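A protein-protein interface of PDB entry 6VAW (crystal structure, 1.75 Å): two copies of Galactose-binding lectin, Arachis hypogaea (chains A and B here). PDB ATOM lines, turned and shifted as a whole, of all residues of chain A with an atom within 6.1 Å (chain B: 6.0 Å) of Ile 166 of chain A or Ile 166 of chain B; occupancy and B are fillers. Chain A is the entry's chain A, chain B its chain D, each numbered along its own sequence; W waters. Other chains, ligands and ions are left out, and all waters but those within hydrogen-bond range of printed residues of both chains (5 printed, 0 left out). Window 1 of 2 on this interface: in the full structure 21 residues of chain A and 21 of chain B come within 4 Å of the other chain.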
ATOM      1  N   PHE A  65     -20.450 -29.521  -5.770  1.00  0.00           N
ATOM      2  CA  PHE A  65     -21.452 -28.768  -5.031  1.00  0.00           C
ATOM      3  C   PHE A  65     -21.728 -27.416  -5.695  1.00  0.00           C
ATOM      4  O   PHE A  65     -20.916 -26.886  -6.474  1.00  0.00           O
ATOM      5  CB  PHE A  65     -21.111 -28.608  -3.541  1.00  0.00           C
ATOM      6  CG  PHE A  65     -19.884 -27.800  -3.208  1.00  0.00           C
ATOM      7  CD1 PHE A  65     -19.916 -26.404  -3.248  1.00  0.00           C
ATOM      8  CD2 PHE A  65     -18.731 -28.421  -2.741  1.00  0.00           C
ATOM      9  CE1 PHE A  65     -18.804 -25.649  -2.883  1.00  0.00           C
ATOM     10  CE2 PHE A  65     -17.606 -27.663  -2.386  1.00  0.00           C
ATOM     11  CZ  PHE A  65     -17.644 -26.291  -2.474  1.00  0.00           C
ATOM     12  N   LEU A  66     -22.927 -26.902  -5.394  1.00  0.00           N
ATOM     13  CA  LEU A  66     -23.434 -25.613  -5.823  1.00  0.00           C
ATOM     14  C   LEU A  66     -23.939 -24.929  -4.562  1.00  0.00           C
ATOM     15  O   LEU A  66     -24.785 -25.493  -3.878  1.00  0.00           O
ATOM     16  CB  LEU A  66     -24.557 -25.746  -6.872  1.00  0.00           C
ATOM     17  CG  LEU A  66     -25.373 -24.467  -7.132  1.00  0.00           C
ATOM     18  CD1 LEU A  66     -24.463 -23.356  -7.785  1.00  0.00           C
ATOM     19  CD2 LEU A  66     -26.585 -24.753  -7.980  1.00  0.00           C
ATOM     20  N   THR A  67     -23.442 -23.735  -4.275  1.00  0.00           N
ATOM     21  CA  THR A  67     -23.920 -23.032  -3.082  1.00  0.00           C
ATOM     22  C   THR A  67     -24.063 -21.566  -3.398  1.00  0.00           C
ATOM     23  O   THR A  67     -23.304 -21.023  -4.186  1.00  0.00           O
ATOM     24  CB  THR A  67     -23.039 -23.308  -1.817  1.00  0.00           C
ATOM     25  OG1 THR A  67     -23.649 -22.720  -0.657  1.00  0.00           O
ATOM     26  CG2 THR A  67     -21.593 -22.823  -1.935  1.00  0.00           C
ATOM     27  N   THR A 164     -22.295 -16.946  -5.608  1.00  0.00           N
ATOM     28  CA  THR A 164     -22.587 -18.261  -6.124  1.00  0.00           C
ATOM     29  C   THR A 164     -21.245 -18.952  -6.263  1.00  0.00           C
ATOM     30  O   THR A 164     -20.295 -18.366  -6.768  1.00  0.00           O
ATOM     31  CB  THR A 164     -23.393 -18.181  -7.433  1.00  0.00           C
ATOM     32  OG1 THR A 164     -24.719 -17.776  -7.126  1.00  0.00           O
ATOM     33  CG2 THR A 164     -23.480 -19.523  -8.145  1.00  0.00           C
ATOM     34  N   VAL A 165     -21.169 -20.183  -5.793  1.00  0.00           N
ATOM     35  CA  VAL A 165     -19.954 -20.967  -5.828  1.00  0.00           C
ATOM     36  C   VAL A 165     -20.261 -22.343  -6.445  1.00  0.00           C
ATOM     37  O   VAL A 165     -21.203 -23.030  -6.062  1.00  0.00           O
ATOM     38  CB  VAL A 165     -19.290 -21.101  -4.430  1.00  0.00           C
ATOM     39  CG1 VAL A 165     -18.005 -21.887  -4.527  1.00  0.00           C
ATOM     40  CG2 VAL A 165     -19.037 -19.737  -3.767  1.00  0.00           C
ATOM     41  N   ILE A 166     -19.401 -22.754  -7.383  1.00  0.00           N
ATOM     42  CA  ILE A 166     -19.523 -24.061  -8.041  1.00  0.00           C
ATOM     43  C   ILE A 166     -18.224 -24.807  -7.828  1.00  0.00           C
ATOM     44  O   ILE A 166     -17.165 -24.296  -8.219  1.00  0.00           O
ATOM     45  CB  ILE A 166     -19.852 -23.991  -9.559  1.00  0.00           C
ATOM     46  CG1 ILE A 166     -21.180 -23.290  -9.859  1.00  0.00           C
ATOM     47  CG2 ILE A 166     -19.819 -25.402 -10.202  1.00  0.00           C
ATOM     48  CD1 ILE A 166     -21.347 -22.974 -11.367  1.00  0.00           C
ATOM     49  N   TYR A 167     -18.305 -26.024  -7.258  1.00  0.00           N
ATOM     50  CA  TYR A 167     -17.120 -26.881  -7.191  1.00  0.00           C
ATOM     51  C   TYR A 167     -17.351 -28.060  -8.124  1.00  0.00           C
ATOM     52  O   TYR A 167     -18.308 -28.820  -7.942  1.00  0.00           O
ATOM     53  CB  TYR A 167     -16.761 -27.325  -5.768  1.00  0.00           C
ATOM     54  CG  TYR A 167     -15.496 -28.154  -5.729  1.00  0.00           C
ATOM     55  CD1 TYR A 167     -14.248 -27.570  -5.954  1.00  0.00           C
ATOM     56  CD2 TYR A 167     -15.550 -29.539  -5.597  1.00  0.00           C
ATOM     57  CE1 TYR A 167     -13.083 -28.338  -5.988  1.00  0.00           C
ATOM     58  CE2 TYR A 167     -14.395 -30.316  -5.623  1.00  0.00           C
ATOM     59  CZ  TYR A 167     -13.159 -29.710  -5.808  1.00  0.00           C
ATOM     60  OH  TYR A 167     -12.001 -30.455  -5.797  1.00  0.00           O
ATOM     61  N   ASP A 168     -16.551 -28.147  -9.185  1.00  0.00           N
ATOM     62  CA  ASP A 168     -16.635 -29.241 -10.154  1.00  0.00           C
ATOM     63  C   ASP A 168     -15.597 -30.313  -9.772  1.00  0.00           C
ATOM     64  O   ASP A 168     -14.403 -30.096  -9.967  1.00  0.00           O
ATOM     65  CB  ASP A 168     -16.388 -28.737 -11.583  1.00  0.00           C
ATOM     66  CG  ASP A 168     -16.384 -29.890 -12.574  1.00  0.00           C
ATOM     67  OD1 ASP A 168     -17.443 -30.534 -12.749  1.00  0.00           O
ATOM     68  OD2 ASP A 168     -15.330 -30.186 -13.116  1.00  0.00           O
ATOM     69  N   THR A 173     -12.119 -27.726  -9.915  1.00  0.00           N
ATOM     70  CA  THR A 173     -12.208 -26.265 -10.010  1.00  0.00           C
ATOM     71  C   THR A 173     -13.252 -25.710  -9.071  1.00  0.00           C
ATOM     72  O   THR A 173     -14.392 -26.160  -9.084  1.00  0.00           O
ATOM     73  CB  THR A 173     -12.507 -25.822 -11.471  1.00  0.00           C
ATOM     74  OG1 THR A 173     -11.475 -26.321 -12.330  1.00  0.00           O
ATOM     75  CG2 THR A 173     -12.598 -24.297 -11.612  1.00  0.00           C
ATOM     76  N   LEU A 174     -12.843 -24.722  -8.263  1.00  0.00           N
ATOM     77  CA  LEU A 174     -13.728 -23.946  -7.399  1.00  0.00           C
ATOM     78  C   LEU A 174     -13.939 -22.586  -8.102  1.00  0.00           C
ATOM     79  O   LEU A 174     -12.979 -21.828  -8.270  1.00  0.00           O
ATOM     80  CB  LEU A 174     -13.078 -23.778  -6.021  1.00  0.00           C
ATOM     81  CG  LEU A 174     -13.868 -23.014  -4.993  1.00  0.00           C
ATOM     82  CD1 LEU A 174     -14.988 -23.824  -4.463  1.00  0.00           C
ATOM     83  CD2 LEU A 174     -12.989 -22.636  -3.765  1.00  0.00           C
ATOM     84  N   SER A 175     -15.141 -22.342  -8.601  1.00  0.00           N
ATOM     85  CA  SER A 175     -15.483 -21.105  -9.308  1.00  0.00           C
ATOM     86  C   SER A 175     -16.414 -20.271  -8.440  1.00  0.00           C
ATOM     87  O   SER A 175     -17.346 -20.814  -7.861  1.00  0.00           O
ATOM     88  CB  SER A 175     -16.100 -21.405 -10.669  1.00  0.00           C
ATOM     89  OG  SER A 175     -16.158 -20.190 -11.389  1.00  0.00           O
ATOM     90  N   VAL A 176     -16.158 -18.968  -8.369  1.00  0.00           N
ATOM     91  CA  VAL A 176     -16.881 -18.005  -7.517  1.00  0.00           C
ATOM     92  C   VAL A 176     -17.354 -16.812  -8.352  1.00  0.00           C
ATOM     93  O   VAL A 176     -16.549 -16.214  -9.075  1.00  0.00           O
ATOM     94  CB  VAL A 176     -15.974 -17.521  -6.344  1.00  0.00           C
ATOM     95  CG1 VAL A 176     -16.720 -16.566  -5.408  1.00  0.00           C
ATOM     96  CG2 VAL A 176     -15.375 -18.685  -5.567  1.00  0.00           C
ATOM     97  N   ALA A 177     -18.633 -16.453  -8.214  1.00  0.00           N
ATOM     98  CA  ALA A 177     -19.209 -15.267  -8.859  1.00  0.00           C
ATOM     99  C   ALA A 177     -19.841 -14.423  -7.760  1.00  0.00           C
ATOM    100  O   ALA A 177     -20.698 -14.920  -7.027  1.00  0.00           O
ATOM    101  CB  ALA A 177     -20.226 -15.636  -9.943  1.00  0.00           C
ATOM    102  N   THR A 187     -15.443 -12.281 -10.564  1.00  0.00           N
ATOM    103  CA  THR A 187     -15.271 -13.733 -10.528  1.00  0.00           C
ATOM    104  C   THR A 187     -13.849 -14.115 -10.176  1.00  0.00           C
ATOM    105  O   THR A 187     -12.910 -13.369 -10.452  1.00  0.00           O
ATOM    106  CB  THR A 187     -15.667 -14.425 -11.871  1.00  0.00           C
ATOM    107  OG1 THR A 187     -14.734 -14.068 -12.894  1.00  0.00           O
ATOM    108  CG2 THR A 187     -17.106 -14.141 -12.314  1.00  0.00           C
ATOM    109  N   PHE B  65     -18.840 -13.720 -16.799  1.00  0.00           N
ATOM    110  CA  PHE B  65     -20.298 -13.669 -16.770  1.00  0.00           C
ATOM    111  C   PHE B  65     -20.858 -14.736 -15.854  1.00  0.00           C
ATOM    112  O   PHE B  65     -20.191 -15.729 -15.544  1.00  0.00           O
ATOM    113  CB  PHE B  65     -20.952 -13.727 -18.168  1.00  0.00           C
ATOM    114  CG  PHE B  65     -20.763 -14.999 -18.943  1.00  0.00           C
ATOM    115  CD1 PHE B  65     -21.522 -16.129 -18.651  1.00  0.00           C
ATOM    116  CD2 PHE B  65     -19.905 -15.044 -20.040  1.00  0.00           C
ATOM    117  CE1 PHE B  65     -21.404 -17.286 -19.423  1.00  0.00           C
ATOM    118  CE2 PHE B  65     -19.781 -16.206 -20.800  1.00  0.00           C
ATOM    119  CZ  PHE B  65     -20.510 -17.327 -20.468  1.00  0.00           C
ATOM    120  N   LEU B  66     -22.087 -14.484 -15.400  1.00  0.00           N
ATOM    121  CA  LEU B  66     -22.885 -15.342 -14.536  1.00  0.00           C
ATOM    122  C   LEU B  66     -24.242 -15.413 -15.156  1.00  0.00           C
ATOM    123  O   LEU B  66     -24.871 -14.379 -15.356  1.00  0.00           O
ATOM    124  CB  LEU B  66     -22.963 -14.805 -13.089  1.00  0.00           C
ATOM    125  CG  LEU B  66     -24.016 -15.486 -12.187  1.00  0.00           C
ATOM    126  CD1 LEU B  66     -23.703 -16.976 -11.975  1.00  0.00           C
ATOM    127  CD2 LEU B  66     -24.161 -14.732 -10.830  1.00  0.00           C
ATOM    128  N   THR B  67     -24.730 -16.607 -15.420  1.00  0.00           N
ATOM    129  CA  THR B  67     -26.058 -16.706 -16.019  1.00  0.00           C
ATOM    130  C   THR B  67     -26.777 -17.893 -15.415  1.00  0.00           C
ATOM    131  O   THR B  67     -26.153 -18.906 -15.100  1.00  0.00           O
ATOM    132  CB  THR B  67     -26.020 -16.731 -17.591  1.00  0.00           C
ATOM    133  OG1 THR B  67     -27.349 -16.700 -18.125  1.00  0.00           O
ATOM    134  CG2 THR B  67     -25.279 -17.950 -18.200  1.00  0.00           C
ATOM    135  N   THR B 164     -26.948 -23.050 -13.766  1.00  0.00           N
ATOM    136  CA  THR B 164     -26.152 -21.893 -13.391  1.00  0.00           C
ATOM    137  C   THR B 164     -24.815 -22.066 -14.138  1.00  0.00           C
ATOM    138  O   THR B 164     -24.256 -23.163 -14.161  1.00  0.00           O
ATOM    139  CB  THR B 164     -26.009 -21.759 -11.870  1.00  0.00           C
ATOM    140  OG1 THR B 164     -27.269 -21.351 -11.331  1.00  0.00           O
ATOM    141  CG2 THR B 164     -24.957 -20.743 -11.479  1.00  0.00           C
ATOM    142  N   VAL B 165     -24.367 -21.009 -14.803  1.00  0.00           N
ATOM    143  CA  VAL B 165     -23.126 -21.023 -15.563  1.00  0.00           C
ATOM    144  C   VAL B 165     -22.249 -19.840 -15.144  1.00  0.00           C
ATOM    145  O   VAL B 165     -22.724 -18.708 -15.101  1.00  0.00           O
ATOM    146  CB  VAL B 165     -23.372 -21.028 -17.093  1.00  0.00           C
ATOM    147  CG1 VAL B 165     -22.060 -21.111 -17.851  1.00  0.00           C
ATOM    148  CG2 VAL B 165     -24.299 -22.160 -17.525  1.00  0.00           C
ATOM    149  N   ILE B 166     -20.961 -20.112 -14.881  1.00  0.00           N
ATOM    150  CA  ILE B 166     -19.975 -19.085 -14.536  1.00  0.00           C
ATOM    151  C   ILE B 166     -18.829 -19.153 -15.554  1.00  0.00           C
ATOM    152  O   ILE B 166     -18.182 -20.201 -15.699  1.00  0.00           O
ATOM    153  CB  ILE B 166     -19.403 -19.176 -13.090  1.00  0.00           C
ATOM    154  CG1 ILE B 166     -20.510 -19.141 -11.979  1.00  0.00           C
ATOM    155  CG2 ILE B 166     -18.333 -18.089 -12.856  1.00  0.00           C
ATOM    156  CD1 ILE B 166     -20.011 -19.586 -10.611  1.00  0.00           C
ATOM    157  N   TYR B 167     -18.514 -18.017 -16.166  1.00  0.00           N
ATOM    158  CA  TYR B 167     -17.310 -17.940 -16.989  1.00  0.00           C
ATOM    159  C   TYR B 167     -16.325 -17.008 -16.268  1.00  0.00           C
ATOM    160  O   TYR B 167     -16.619 -15.828 -16.101  1.00  0.00           O
ATOM    161  CB  TYR B 167     -17.576 -17.496 -18.420  1.00  0.00           C
ATOM    162  CG  TYR B 167     -16.317 -17.491 -19.255  1.00  0.00           C
ATOM    163  CD1 TYR B 167     -15.693 -18.685 -19.622  1.00  0.00           C
ATOM    164  CD2 TYR B 167     -15.677 -16.296 -19.575  1.00  0.00           C
ATOM    165  CE1 TYR B 167     -14.492 -18.686 -20.336  1.00  0.00           C
ATOM    166  CE2 TYR B 167     -14.481 -16.286 -20.301  1.00  0.00           C
ATOM    167  CZ  TYR B 167     -13.898 -17.485 -20.682  1.00  0.00           C
ATOM    168  OH  TYR B 167     -12.740 -17.504 -21.425  1.00  0.00           O
ATOM    169  N   ASP B 168     -15.177 -17.552 -15.831  1.00  0.00           N
ATOM    170  CA  ASP B 168     -14.130 -16.777 -15.169  1.00  0.00           C
ATOM    171  C   ASP B 168     -13.070 -16.402 -16.205  1.00  0.00           C
ATOM    172  O   ASP B 168     -12.303 -17.277 -16.621  1.00  0.00           O
ATOM    173  CB  ASP B 168     -13.508 -17.566 -14.030  1.00  0.00           C
ATOM    174  CG  ASP B 168     -12.350 -16.813 -13.408  1.00  0.00           C
ATOM    175  OD1 ASP B 168     -12.594 -15.753 -12.797  1.00  0.00           O
ATOM    176  OD2 ASP B 168     -11.208 -17.249 -13.584  1.00  0.00           O
ATOM    177  N   THR B 173     -12.119 -20.375 -17.573  1.00  0.00           N
ATOM    178  CA  THR B 173     -12.909 -21.551 -17.194  1.00  0.00           C
ATOM    179  C   THR B 173     -14.388 -21.294 -17.285  1.00  0.00           C
ATOM    180  O   THR B 173     -14.868 -20.347 -16.685  1.00  0.00           O
ATOM    181  CB  THR B 173     -12.571 -22.020 -15.764  1.00  0.00           C
ATOM    182  OG1 THR B 173     -11.171 -22.324 -15.710  1.00  0.00           O
ATOM    183  CG2 THR B 173     -13.409 -23.235 -15.338  1.00  0.00           C
ATOM    184  N   LEU B 174     -15.084 -22.183 -17.997  1.00  0.00           N
ATOM    185  CA  LEU B 174     -16.547 -22.246 -18.119  1.00  0.00           C
ATOM    186  C   LEU B 174     -17.010 -23.357 -17.147  1.00  0.00           C
ATOM    187  O   LEU B 174     -16.567 -24.515 -17.267  1.00  0.00           O
ATOM    188  CB  LEU B 174     -16.963 -22.544 -19.570  1.00  0.00           C
ATOM    189  CG  LEU B 174     -18.463 -22.414 -19.880  1.00  0.00           C
ATOM    190  CD1 LEU B 174     -18.952 -20.985 -19.677  1.00  0.00           C
ATOM    191  CD2 LEU B 174     -18.783 -22.882 -21.310  1.00  0.00           C
ATOM    192  N   SER B 175     -17.760 -22.966 -16.103  1.00  0.00           N
ATOM    193  CA  SER B 175     -18.277 -23.924 -15.104  1.00  0.00           C
ATOM    194  C   SER B 175     -19.807 -23.957 -15.171  1.00  0.00           C
ATOM    195  O   SER B 175     -20.452 -22.902 -15.245  1.00  0.00           O
ATOM    196  CB  SER B 175     -17.809 -23.558 -13.701  1.00  0.00           C
ATOM    197  OG  SER B 175     -16.400 -23.591 -13.580  1.00  0.00           O
ATOM    198  N   VAL B 176     -20.388 -25.172 -15.133  1.00  0.00           N
ATOM    199  CA  VAL B 176     -21.828 -25.410 -15.259  1.00  0.00           C
ATOM    200  C   VAL B 176     -22.328 -26.287 -14.102  1.00  0.00           C
ATOM    201  O   VAL B 176     -21.712 -27.323 -13.809  1.00  0.00           O
ATOM    202  CB  VAL B 176     -22.131 -26.101 -16.624  1.00  0.00           C
ATOM    203  CG1 VAL B 176     -23.623 -26.312 -16.843  1.00  0.00           C
ATOM    204  CG2 VAL B 176     -21.515 -25.348 -17.808  1.00  0.00           C
ATOM    205  N   ALA B 177     -23.415 -25.867 -13.450  1.00  0.00           N
ATOM    206  CA  ALA B 177     -24.100 -26.658 -12.407  1.00  0.00           C
ATOM    207  C   ALA B 177     -25.557 -26.810 -12.833  1.00  0.00           C
ATOM    208  O   ALA B 177     -26.252 -25.816 -13.100  1.00  0.00           O
ATOM    209  CB  ALA B 177     -23.973 -26.014 -11.017  1.00  0.00           C
ATOM    210  N   THR B 187     -22.305 -31.399 -12.475  1.00  0.00           N
ATOM    211  CA  THR B 187     -21.413 -30.288 -12.838  1.00  0.00           C
ATOM    212  C   THR B 187     -20.489 -30.700 -13.966  1.00  0.00           C
ATOM    213  O   THR B 187     -20.168 -31.888 -14.121  1.00  0.00           O
ATOM    214  CB  THR B 187     -20.579 -29.752 -11.650  1.00  0.00           C
ATOM    215  OG1 THR B 187     -19.640 -30.746 -11.233  1.00  0.00           O
ATOM    216  CG2 THR B 187     -21.424 -29.270 -10.485  1.00  0.00           C
HETATM  217  O   HOH W   1     -15.571 -20.950 -13.845  1.00  0.00           O
HETATM  218  O   HOH W   2      -9.863 -24.425 -14.561  1.00  0.00           O
HETATM  219  O   HOH W   3     -11.573 -13.496 -13.897  1.00  0.00           O
HETATM  220  O   HOH W   4     -17.445 -33.152 -11.963  1.00  0.00           O
HETATM  221  O   HOH W   5     -16.140 -25.000 -11.194  1.00  0.00           O
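The side-chain carboxylate (OD1) of Asp 168 of chain A is in hydrogen-bond range of the side-chain hydroxyl (OG1) of Thr 187 of chain B, at 2.7 Å. OG1 of Thr 187 of chain A sits at hydrogen-bond distance from OD1 of Asp 168 of chain B.
Among the printed residues, pairs that only touch across the chains: Thr 164 of chain A with Thr 164 of chain B (3.8 Å), Ile 166 of chain A with Ile 166 of chain B (3.7 Å), Ile 166 of chain A with Ser 175 of chain B (3.98 Å), Thr 173 of chain A with Thr 173 of chain B (3.96 Å), Ser 175 of chain A with Ile 166 of chain B (3.4 Å) and Ser 175 of chain A with Ser 175 of chain B (3.7 Å).
Of the printed residues of chain B, Ile 166 of chain A touches Ile 166 and Ser 175. Of the printed residues of chain A, Ile 166 of chain B touches Ile 166 (3.7 Å) and Ser 175 (3.4 Å). Of the printed residues of chain B, Thr 164 of chain A touches Thr 164 (3.8 Å). Of the printed residues of chain B, Thr 173 of chain A touches Thr 173 (3.96 Å). Thr 67 of chain B touches none of the printed residues of chain A. Leu 66 of chain B touches none of the printed residues of chain A. The nearest printed residue of chain B that does not touch Ile 166 of chain A is Ala 177 of chain B (4.03 Å). The nearest printed residue of chain A that does not touch Ile 166 of chain B is Ala 177 of chain A (4.01 Å).
Thr 164 of chain A touches its own counterpart, Thr 164 of chain B. Ile 166 of chain A touches Ser 175 of chain B, and with the chains exchanged Ser 175 of chain A touches Ile 166 of chain B. Asp 168 of chain A touches Thr 187 of chain B, and with the chains exchanged Thr 187 of chain A touches Asp 168 of chain B. Thr 173 of chain A touches its own counterpart, Thr 173 of chain B. Positions printed for both chains: 65, 66, 67, 164, 165, 166, 167, 168, 173, 174, 175, 176, 177 and 187. Of the 8 pairs that touch across the chains among the printed residues, 8 have their exchanged pair printed and touching as well.
Water W1 lies within hydrogen-bond range of OG of Ser 175 of chain A (2.6 Å), OG of Ser 175 of chain B (2.8 Å), O of Thr 173 of chain B (3.0 Å) and O of Ile 166 of chain B (3.3 Å). Water W3 lies within hydrogen-bond range of OD1 of Asp 168 of chain B and OG1 of Thr 187 of chain A. Water W2 bridges the side-chain hydroxyl (OG1) of Thr 173 of chain B (2.7 Å) and the side-chain hydroxyl (OG1) of Thr 173 of chain A (3.3 Å). Water W4 bridges the side-chain carboxylate (OD1) of Asp 168 of chain A (2.7 Å) and the side-chain hydroxyl (OG1) of Thr 187 of chain B (3.3 Å). Water W5 lies within hydrogen-bond range of the side-chain hydroxyl (OG) of Ser 175 of chain B (2.8 Å), the backbone carbonyl oxygen (O) of Thr 173 of chain A (3.0 Å) and the backbone carbonyl oxygen (O) of Ile 166 of chain A (3.2 Å).
Among the printed residues, 8 pairs touch across the chains.
The backbone NH (N) of Ala 177 of chain A sits at hydrogen-bond distance from the backbone carbonyl oxygen (O) of Thr 164 of chain A. N of Ser 175 of chain A sits at hydrogen-bond distance from O of Ile 166 of chain A (2.8 Å). The backbone NH (N) of Asp 168 of chain A is in hydrogen-bond range of the backbone carbonyl oxygen (O) of Thr 173 of chain A (2.9 Å). The backbone NH (N) of Ala 177 of chain B sits at hydrogen-bond distance from the backbone carbonyl oxygen (O) of Thr 164 of chain B (2.9 Å). The backbone carbonyl oxygen of Ile 166 of chain B lies within hydrogen-bond range of the backbone NH of Ser 175 of chain B (2.8 Å). O of Thr 173 of chain B sits at hydrogen-bond distance from N of Asp 168 of chain B, at 2.9 Å.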
